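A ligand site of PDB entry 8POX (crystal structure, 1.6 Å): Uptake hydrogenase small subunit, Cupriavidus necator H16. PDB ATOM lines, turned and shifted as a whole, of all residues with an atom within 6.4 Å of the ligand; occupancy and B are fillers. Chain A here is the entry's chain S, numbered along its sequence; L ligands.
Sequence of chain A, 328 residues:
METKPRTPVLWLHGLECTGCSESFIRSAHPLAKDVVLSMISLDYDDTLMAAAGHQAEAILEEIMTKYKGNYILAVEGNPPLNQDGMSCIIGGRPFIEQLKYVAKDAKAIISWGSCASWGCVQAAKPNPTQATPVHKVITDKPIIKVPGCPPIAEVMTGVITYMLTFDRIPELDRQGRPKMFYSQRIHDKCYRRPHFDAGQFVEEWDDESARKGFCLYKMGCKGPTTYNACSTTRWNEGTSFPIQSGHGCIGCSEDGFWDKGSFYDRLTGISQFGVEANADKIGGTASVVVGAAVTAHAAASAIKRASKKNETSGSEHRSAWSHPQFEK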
ATOM      1  N   ILE A 186      -8.401  -7.291 -20.115  1.00  0.00           N
ATOM      2  CA  ILE A 186      -9.800  -6.868 -19.939  1.00  0.00           C
ATOM      3  C   ILE A 186     -10.530  -7.879 -19.043  1.00  0.00           C
ATOM      4  O   ILE A 186     -11.250  -7.499 -18.112  1.00  0.00           O
ATOM      5  CB  ILE A 186     -10.565  -6.791 -21.282  1.00  0.00           C
ATOM      6  CG1 ILE A 186      -9.815  -5.953 -22.321  1.00  0.00           C
ATOM      7  CG2 ILE A 186     -11.965  -6.230 -21.072  1.00  0.00           C
ATOM      8  CD1 ILE A 186      -9.497  -4.542 -21.875  1.00  0.00           C
ATOM      9  N   HIS A 187     -10.292  -9.157 -19.327  1.00  0.00           N
ATOM     10  CA  HIS A 187     -10.994 -10.287 -18.699  1.00  0.00           C
ATOM     11  C   HIS A 187     -10.671 -10.445 -17.206  1.00  0.00           C
ATOM     12  O   HIS A 187     -11.432 -11.096 -16.481  1.00  0.00           O
ATOM     13  CB  HIS A 187     -10.598 -11.551 -19.474  1.00  0.00           C
ATOM     14  CG  HIS A 187     -11.284 -12.809 -19.048  1.00  0.00           C
ATOM     15  ND1 HIS A 187     -12.573 -13.113 -19.419  1.00  0.00           N
ATOM     16  CD2 HIS A 187     -10.824 -13.892 -18.374  1.00  0.00           C
ATOM     17  CE1 HIS A 187     -12.891 -14.307 -18.965  1.00  0.00           C
ATOM     18  NE2 HIS A 187     -11.853 -14.800 -18.316  1.00  0.00           N
ATOM     19  N   ASP A 188      -9.555  -9.869 -16.752  1.00  0.00           N
ATOM     20  CA  ASP A 188      -9.156 -10.007 -15.342  1.00  0.00           C
ATOM     21  C   ASP A 188     -10.221  -9.454 -14.390  1.00  0.00           C
ATOM     22  O   ASP A 188     -10.586 -10.122 -13.413  1.00  0.00           O
ATOM     23  CB  ASP A 188      -7.822  -9.303 -15.056  1.00  0.00           C
ATOM     24  CG  ASP A 188      -6.628 -10.013 -15.691  1.00  0.00           C
ATOM     25  OD1 ASP A 188      -6.753 -11.180 -16.117  1.00  0.00           O
ATOM     26  OD2 ASP A 188      -5.532  -9.401 -15.743  1.00  0.00           O
ATOM     27  N   CYS A 190     -13.196  -7.625 -15.691  1.00  0.00           N
ATOM     28  CA  CYS A 190     -14.469  -7.377 -16.388  1.00  0.00           C
ATOM     29  C   CYS A 190     -15.648  -7.731 -15.495  1.00  0.00           C
ATOM     30  O   CYS A 190     -15.697  -8.822 -14.938  1.00  0.00           O
ATOM     31  CB  CYS A 190     -14.549  -8.210 -17.669  1.00  0.00           C
ATOM     32  SG  CYS A 190     -16.124  -8.051 -18.548  1.00  0.00           S
ATOM     33  N   TYR A 191     -16.608  -6.811 -15.367  1.00  0.00           N
ATOM     34  CA  TYR A 191     -17.761  -7.000 -14.500  1.00  0.00           C
ATOM     35  C   TYR A 191     -18.665  -8.167 -14.943  1.00  0.00           C
ATOM     36  O   TYR A 191     -19.482  -8.621 -14.151  1.00  0.00           O
ATOM     37  CB  TYR A 191     -18.582  -5.701 -14.368  1.00  0.00           C
ATOM     38  CG  TYR A 191     -19.538  -5.497 -15.521  1.00  0.00           C
ATOM     39  CD1 TYR A 191     -19.064  -5.098 -16.779  1.00  0.00           C
ATOM     40  CD2 TYR A 191     -20.893  -5.720 -15.382  1.00  0.00           C
ATOM     41  CE1 TYR A 191     -19.924  -4.937 -17.840  1.00  0.00           C
ATOM     42  CE2 TYR A 191     -21.761  -5.561 -16.449  1.00  0.00           C
ATOM     43  CZ  TYR A 191     -21.267  -5.162 -17.667  1.00  0.00           C
ATOM     44  OH  TYR A 191     -22.116  -5.007 -18.724  1.00  0.00           O
ATOM     45  N   ARG A 192     -18.518  -8.646 -16.174  1.00  0.00           N
ATOM     46  CA  ARG A 192     -19.266  -9.840 -16.620  1.00  0.00           C
ATOM     47  C   ARG A 192     -18.584 -11.170 -16.245  1.00  0.00           C
ATOM     48  O   ARG A 192     -19.103 -12.234 -16.549  1.00  0.00           O
ATOM     49  CB  ARG A 192     -19.522  -9.791 -18.141  1.00  0.00           C
ATOM     50  CG  ARG A 192     -20.327  -8.563 -18.572  1.00  0.00           C
ATOM     51  CD  ARG A 192     -20.945  -8.726 -19.946  1.00  0.00           C
ATOM     52  NE  ARG A 192     -21.691  -7.525 -20.328  1.00  0.00           N
ATOM     53  CZ  ARG A 192     -22.669  -7.475 -21.237  1.00  0.00           C
ATOM     54  NH1 ARG A 192     -23.086  -8.565 -21.867  1.00  0.00           N
ATOM     55  NH2 ARG A 192     -23.259  -6.306 -21.506  1.00  0.00           N
ATOM     56  N   ARG A 193     -17.434 -11.111 -15.570  1.00  0.00           N
ATOM     57  CA  ARG A 193     -16.712 -12.331 -15.202  1.00  0.00           C
ATOM     58  C   ARG A 193     -17.521 -13.366 -14.411  1.00  0.00           C
ATOM     59  O   ARG A 193     -17.353 -14.554 -14.640  1.00  0.00           O
ATOM     60  CB  ARG A 193     -15.424 -12.027 -14.425  1.00  0.00           C
ATOM     61  CG  ARG A 193     -14.190 -11.877 -15.298  1.00  0.00           C
ATOM     62  CD  ARG A 193     -13.849 -13.150 -16.049  1.00  0.00           C
ATOM     63  NE  ARG A 193     -13.434 -14.260 -15.196  1.00  0.00           N
ATOM     64  CZ  ARG A 193     -12.190 -14.464 -14.756  1.00  0.00           C
ATOM     65  NH1 ARG A 193     -11.209 -13.614 -15.059  1.00  0.00           N
ATOM     66  NH2 ARG A 193     -11.910 -15.514 -14.000  1.00  0.00           N
ATOM     67  N   PRO A 194     -18.365 -12.923 -13.463  1.00  0.00           N
ATOM     68  CA  PRO A 194     -19.148 -13.938 -12.762  1.00  0.00           C
ATOM     69  C   PRO A 194     -20.060 -14.753 -13.692  1.00  0.00           C
ATOM     70  O   PRO A 194     -20.320 -15.914 -13.418  1.00  0.00           O
ATOM     71  CB  PRO A 194     -19.962 -13.123 -11.754  1.00  0.00           C
ATOM     72  CG  PRO A 194     -19.119 -11.923 -11.491  1.00  0.00           C
ATOM     73  CD  PRO A 194     -18.463 -11.605 -12.816  1.00  0.00           C
ATOM     74  N   HIS A 195     -20.498 -14.171 -14.802  1.00  0.00           N
ATOM     75  CA  HIS A 195     -21.245 -14.937 -15.807  1.00  0.00           C
ATOM     76  C   HIS A 195     -20.321 -15.901 -16.572  1.00  0.00           C
ATOM     77  O   HIS A 195     -20.666 -17.066 -16.762  1.00  0.00           O
ATOM     78  CB  HIS A 195     -22.002 -14.009 -16.760  1.00  0.00           C
ATOM     79  CG  HIS A 195     -23.050 -13.184 -16.085  1.00  0.00           C
ATOM     80  ND1 HIS A 195     -24.101 -13.749 -15.389  1.00  0.00           N
ATOM     81  CD2 HIS A 195     -23.214 -11.843 -15.981  1.00  0.00           C
ATOM     82  CE1 HIS A 195     -24.864 -12.787 -14.886  1.00  0.00           C
ATOM     83  NE2 HIS A 195     -24.344 -11.623 -15.236  1.00  0.00           N
ATOM     84  N   PHE A 196     -19.155 -15.423 -16.989  1.00  0.00           N
ATOM     85  CA  PHE A 196     -18.147 -16.301 -17.613  1.00  0.00           C
ATOM     86  C   PHE A 196     -17.800 -17.486 -16.714  1.00  0.00           C
ATOM     87  O   PHE A 196     -17.759 -18.628 -17.160  1.00  0.00           O
ATOM     88  CB  PHE A 196     -16.863 -15.521 -17.923  1.00  0.00           C
ATOM     89  CG  PHE A 196     -15.756 -16.390 -18.477  1.00  0.00           C
ATOM     90  CD1 PHE A 196     -15.620 -16.587 -19.842  1.00  0.00           C
ATOM     91  CD2 PHE A 196     -14.845 -17.010 -17.626  1.00  0.00           C
ATOM     92  CE1 PHE A 196     -14.610 -17.376 -20.352  1.00  0.00           C
ATOM     93  CE2 PHE A 196     -13.833 -17.802 -18.123  1.00  0.00           C
ATOM     94  CZ  PHE A 196     -13.713 -17.982 -19.490  1.00  0.00           C
ATOM     95  N   PHE A 201     -23.585 -17.311 -21.025  1.00  0.00           N
ATOM     96  CA  PHE A 201     -23.139 -16.653 -22.243  1.00  0.00           C
ATOM     97  C   PHE A 201     -24.277 -16.182 -23.152  1.00  0.00           C
ATOM     98  O   PHE A 201     -25.289 -16.866 -23.307  1.00  0.00           O
ATOM     99  CB  PHE A 201     -22.301 -17.634 -23.060  1.00  0.00           C
ATOM    100  CG  PHE A 201     -21.079 -18.132 -22.359  1.00  0.00           C
ATOM    101  CD1 PHE A 201     -19.984 -17.302 -22.178  1.00  0.00           C
ATOM    102  CD2 PHE A 201     -21.015 -19.442 -21.896  1.00  0.00           C
ATOM    103  CE1 PHE A 201     -18.851 -17.763 -21.527  1.00  0.00           C
ATOM    104  CE2 PHE A 201     -19.876 -19.899 -21.254  1.00  0.00           C
ATOM    105  CZ  PHE A 201     -18.798 -19.066 -21.069  1.00  0.00           C
ATOM    106  N   PHE A 214     -25.080 -11.196 -19.822  1.00  0.00           N
ATOM    107  CA  PHE A 214     -24.247 -12.389 -19.746  1.00  0.00           C
ATOM    108  C   PHE A 214     -22.935 -12.180 -20.524  1.00  0.00           C
ATOM    109  O   PHE A 214     -22.815 -11.265 -21.350  1.00  0.00           O
ATOM    110  CB  PHE A 214     -25.009 -13.620 -20.260  1.00  0.00           C
ATOM    111  CG  PHE A 214     -25.934 -14.267 -19.236  1.00  0.00           C
ATOM    112  CD1 PHE A 214     -26.324 -13.602 -18.080  1.00  0.00           C
ATOM    113  CD2 PHE A 214     -26.437 -15.540 -19.470  1.00  0.00           C
ATOM    114  CE1 PHE A 214     -27.176 -14.215 -17.159  1.00  0.00           C
ATOM    115  CE2 PHE A 214     -27.283 -16.149 -18.556  1.00  0.00           C
ATOM    116  CZ  PHE A 214     -27.657 -15.487 -17.404  1.00  0.00           C
ATOM    117  N   CYS A 215     -21.945 -13.017 -20.247  1.00  0.00           N
ATOM    118  CA  CYS A 215     -20.613 -12.904 -20.853  1.00  0.00           C
ATOM    119  C   CYS A 215     -20.667 -12.963 -22.375  1.00  0.00           C
ATOM    120  O   CYS A 215     -21.513 -13.667 -22.954  1.00  0.00           O
ATOM    121  CB  CYS A 215     -19.720 -14.015 -20.313  1.00  0.00           C
ATOM    122  SG  CYS A 215     -18.120 -14.158 -21.126  1.00  0.00           S
ATOM    123  N   LEU A 216     -19.750 -12.238 -23.010  1.00  0.00           N
ATOM    124  CA  LEU A 216     -19.722 -12.079 -24.480  1.00  0.00           C
ATOM    125  C   LEU A 216     -18.676 -12.955 -25.183  1.00  0.00           C
ATOM    126  O   LEU A 216     -18.427 -12.796 -26.389  1.00  0.00           O
ATOM    127  CB  LEU A 216     -19.514 -10.606 -24.847  1.00  0.00           C
ATOM    128  CG  LEU A 216     -20.667  -9.694 -24.431  1.00  0.00           C
ATOM    129  CD1 LEU A 216     -20.253  -8.234 -24.511  1.00  0.00           C
ATOM    130  CD2 LEU A 216     -21.913  -9.939 -25.280  1.00  0.00           C
ATOM    131  N   TYR A 217     -18.099 -13.913 -24.470  1.00  0.00           N
ATOM    132  CA  TYR A 217     -17.066 -14.806 -25.020  1.00  0.00           C
ATOM    133  C   TYR A 217     -17.485 -15.516 -26.302  1.00  0.00           C
ATOM    134  O   TYR A 217     -16.748 -15.553 -27.277  1.00  0.00           O
ATOM    135  CB  TYR A 217     -16.670 -15.852 -23.988  1.00  0.00           C
ATOM    136  CG  TYR A 217     -15.499 -16.729 -24.373  1.00  0.00           C
ATOM    137  CD1 TYR A 217     -15.677 -17.918 -25.069  1.00  0.00           C
ATOM    138  CD2 TYR A 217     -14.198 -16.387 -23.999  1.00  0.00           C
ATOM    139  CE1 TYR A 217     -14.610 -18.732 -25.397  1.00  0.00           C
ATOM    140  CE2 TYR A 217     -13.118 -17.182 -24.335  1.00  0.00           C
ATOM    141  CZ  TYR A 217     -13.329 -18.365 -25.024  1.00  0.00           C
ATOM    142  OH  TYR A 217     -12.261 -19.166 -25.358  1.00  0.00           O
ATOM    143  N   LYS A 218     -18.672 -16.141 -26.279  1.00  0.00           N
ATOM    144  CA  LYS A 218     -19.172 -16.867 -27.454  1.00  0.00           C
ATOM    145  C   LYS A 218     -19.640 -15.963 -28.608  1.00  0.00           C
ATOM    146  O   LYS A 218     -19.927 -16.461 -29.704  1.00  0.00           O
ATOM    147  CB  LYS A 218     -20.271 -17.854 -27.039  1.00  0.00           C
ATOM    148  CG  LYS A 218     -19.758 -18.891 -26.056  1.00  0.00           C
ATOM    149  CD  LYS A 218     -20.813 -19.907 -25.667  1.00  0.00           C
ATOM    150  CE  LYS A 218     -20.180 -21.044 -24.894  1.00  0.00           C
ATOM    151  NZ  LYS A 218     -21.188 -22.050 -24.455  1.00  0.00           N
ATOM    152  N   CYS A 221     -15.767 -12.094 -27.928  1.00  0.00           N
ATOM    153  CA  CYS A 221     -15.017 -11.187 -27.042  1.00  0.00           C
ATOM    154  C   CYS A 221     -13.551 -11.610 -26.926  1.00  0.00           C
ATOM    155  O   CYS A 221     -13.263 -12.739 -26.560  1.00  0.00           O
ATOM    156  CB  CYS A 221     -15.639 -11.122 -25.650  1.00  0.00           C
ATOM    157  SG  CYS A 221     -14.840  -9.884 -24.583  1.00  0.00           S
ATOM    158  N   LYS A 222     -12.643 -10.693 -27.229  1.00  0.00           N
ATOM    159  CA  LYS A 222     -11.210 -10.959 -27.129  1.00  0.00           C
ATOM    160  C   LYS A 222     -10.611 -10.404 -25.836  1.00  0.00           C
ATOM    161  O   LYS A 222      -9.391 -10.306 -25.698  1.00  0.00           O
ATOM    162  CB  LYS A 222     -10.477 -10.422 -28.365  1.00  0.00           C
ATOM    163  CG  LYS A 222     -10.951 -11.026 -29.681  1.00  0.00           C
ATOM    164  CD  LYS A 222     -11.049 -12.550 -29.610  1.00  0.00           C
ATOM    165  CE  LYS A 222     -11.310 -13.193 -30.963  1.00  0.00           C
ATOM    166  NZ  LYS A 222     -12.549 -12.700 -31.626  1.00  0.00           N
ATOM    167  N   GLY A 223     -11.471 -10.072 -24.879  1.00  0.00           N
ATOM    168  CA  GLY A 223     -11.003  -9.616 -23.567  1.00  0.00           C
ATOM    169  C   GLY A 223     -10.006 -10.531 -22.881  1.00  0.00           C
ATOM    170  O   GLY A 223      -9.081 -10.046 -22.209  1.00  0.00           O
ATOM    171  N   PRO A 224     -10.171 -11.858 -23.025  1.00  0.00           N
ATOM    172  CA  PRO A 224      -9.217 -12.780 -22.397  1.00  0.00           C
ATOM    173  C   PRO A 224      -7.766 -12.686 -22.868  1.00  0.00           C
ATOM    174  O   PRO A 224      -6.888 -13.138 -22.134  1.00  0.00           O
ATOM    175  CB  PRO A 224      -9.799 -14.152 -22.710  1.00  0.00           C
ATOM    176  CG  PRO A 224     -11.266 -13.908 -22.778  1.00  0.00           C
ATOM    177  CD  PRO A 224     -11.372 -12.586 -23.484  1.00  0.00           C
ATOM    178  N   PHE A 241     -17.662   0.964 -21.330  1.00  0.00           N
ATOM    179  CA  PHE A 241     -16.622   0.388 -22.180  1.00  0.00           C
ATOM    180  C   PHE A 241     -17.304  -0.622 -23.114  1.00  0.00           C
ATOM    181  O   PHE A 241     -18.492  -0.921 -22.944  1.00  0.00           O
ATOM    182  CB  PHE A 241     -15.444  -0.202 -21.359  1.00  0.00           C
ATOM    183  CG  PHE A 241     -15.734  -1.488 -20.633  1.00  0.00           C
ATOM    184  CD1 PHE A 241     -16.626  -1.532 -19.569  1.00  0.00           C
ATOM    185  CD2 PHE A 241     -15.011  -2.640 -20.923  1.00  0.00           C
ATOM    186  CE1 PHE A 241     -16.848  -2.703 -18.868  1.00  0.00           C
ATOM    187  CE2 PHE A 241     -15.222  -3.817 -20.218  1.00  0.00           C
ATOM    188  CZ  PHE A 241     -16.148  -3.848 -19.182  1.00  0.00           C
ATOM    189  N   ILE A 243     -17.692  -3.773 -23.625  1.00  0.00           N
ATOM    190  CA  ILE A 243     -18.431  -4.888 -23.039  1.00  0.00           C
ATOM    191  C   ILE A 243     -19.668  -4.424 -22.249  1.00  0.00           C
ATOM    192  O   ILE A 243     -20.741  -5.023 -22.358  1.00  0.00           O
ATOM    193  CB  ILE A 243     -17.501  -5.770 -22.184  1.00  0.00           C
ATOM    194  CG1 ILE A 243     -16.558  -6.541 -23.122  1.00  0.00           C
ATOM    195  CG2 ILE A 243     -18.292  -6.721 -21.284  1.00  0.00           C
ATOM    196  CD1 ILE A 243     -15.187  -6.841 -22.544  1.00  0.00           C
ATOM    197  N   GLY A 248     -18.485  -7.395 -27.629  1.00  0.00           N
ATOM    198  CA  GLY A 248     -17.222  -7.955 -27.169  1.00  0.00           C
ATOM    199  C   GLY A 248     -16.048  -7.053 -27.500  1.00  0.00           C
ATOM    200  O   GLY A 248     -16.072  -6.279 -28.456  1.00  0.00           O
ATOM    201  N   CYS A 249     -15.025  -7.133 -26.669  1.00  0.00           N
ATOM    202  CA  CYS A 249     -13.726  -6.566 -27.004  1.00  0.00           C
ATOM    203  C   CYS A 249     -13.284  -7.141 -28.353  1.00  0.00           C
ATOM    204  O   CYS A 249     -13.454  -8.336 -28.601  1.00  0.00           O
ATOM    205  CB  CYS A 249     -12.727  -6.887 -25.896  1.00  0.00           C
ATOM    206  SG  CYS A 249     -11.036  -6.363 -26.178  1.00  0.00           S
HETATM  207 FE1  LIG L   1     -15.251 -10.712 -22.423  1.00  0.00          FE
HETATM  208 FE2  LIG L   1     -16.750 -12.327 -20.823  1.00  0.00          FE
HETATM  209 FE3  LIG L   1     -15.861  -9.928 -19.933  1.00  0.00          FE
HETATM  210 FE4  LIG L   1     -14.132 -11.982 -20.284  1.00  0.00          FE
HETATM  211  S1  LIG L   1     -15.871 -11.909 -18.787  1.00  0.00           S
HETATM  212  S2  LIG L   1     -13.795  -9.824 -20.936  1.00  0.00           S
HETATM  213  S3  LIG L   1     -14.996 -12.942 -22.230  1.00  0.00           S
HETATM  214  S4  LIG L   1     -17.394 -10.269 -21.614  1.00  0.00           S
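The side-chain sulfur (SG) of Cys 215 binds an iron atom (FE2) of the ligand (2.3 Å).
A sulfur (S1) of the ligand sits close to the backbone NH (N) of Arg 193, 3.7 Å away.
SG of Cys 221 is bound to FE1 of the ligand (2.3 Å).
SG of Cys 190 is bound to FE3 of the ligand (2.3 Å).
The backbone NH (N) of Leu 216 lies close to a sulfur (S4) of the ligand (3.4 Å).
A ring nitrogen (ND1) of His 187 is bound to an iron atom (FE4) of the ligand (2.1 Å).
Merely in contact with the ligand: Ile 243, Tyr 217, Arg 192, Gly 223, Phe 196 and Pro 224.
Within 4 Å of the ligand: His 187, Cys 190, Arg 192, Arg 193, Phe 196, Cys 215, Leu 216, Tyr 217, Cys 221, Gly 223, Pro 224 and Ile 243.
The nearest printed residue that does not touch the ligand is Ile 186 (4.04 Å).
SG of Cys 190 sits close to N of Arg 192, 3.4 Å away.
The guanidinium group (NH1) of Arg 192 is in hydrogen-bond range of the backbone carbonyl oxygen (O) of Phe 214.
N of Gly 223 lies close to SG of Cys 221 (3.4 Å).
The side-chain sulfur (SG) of Cys 215 sits close to the backbone NH (N) of Tyr 217 (3.4 Å).
The backbone carbonyl oxygen (O) of Gly 223 lies within hydrogen-bond range of the backbone NH (N) of His 187 (3.3 Å).
The backbone NH (N) of Cys 249 sits close to the side-chain sulfur (SG) of Cys 221 (3.5 Å).
N of Cys 221 lies within hydrogen-bond range of O of Leu 216.
The backbone carbonyl oxygen (O) of His 187 sits at hydrogen-bond distance from the guanidinium group (NH1) of Arg 193, 2.9 Å away.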
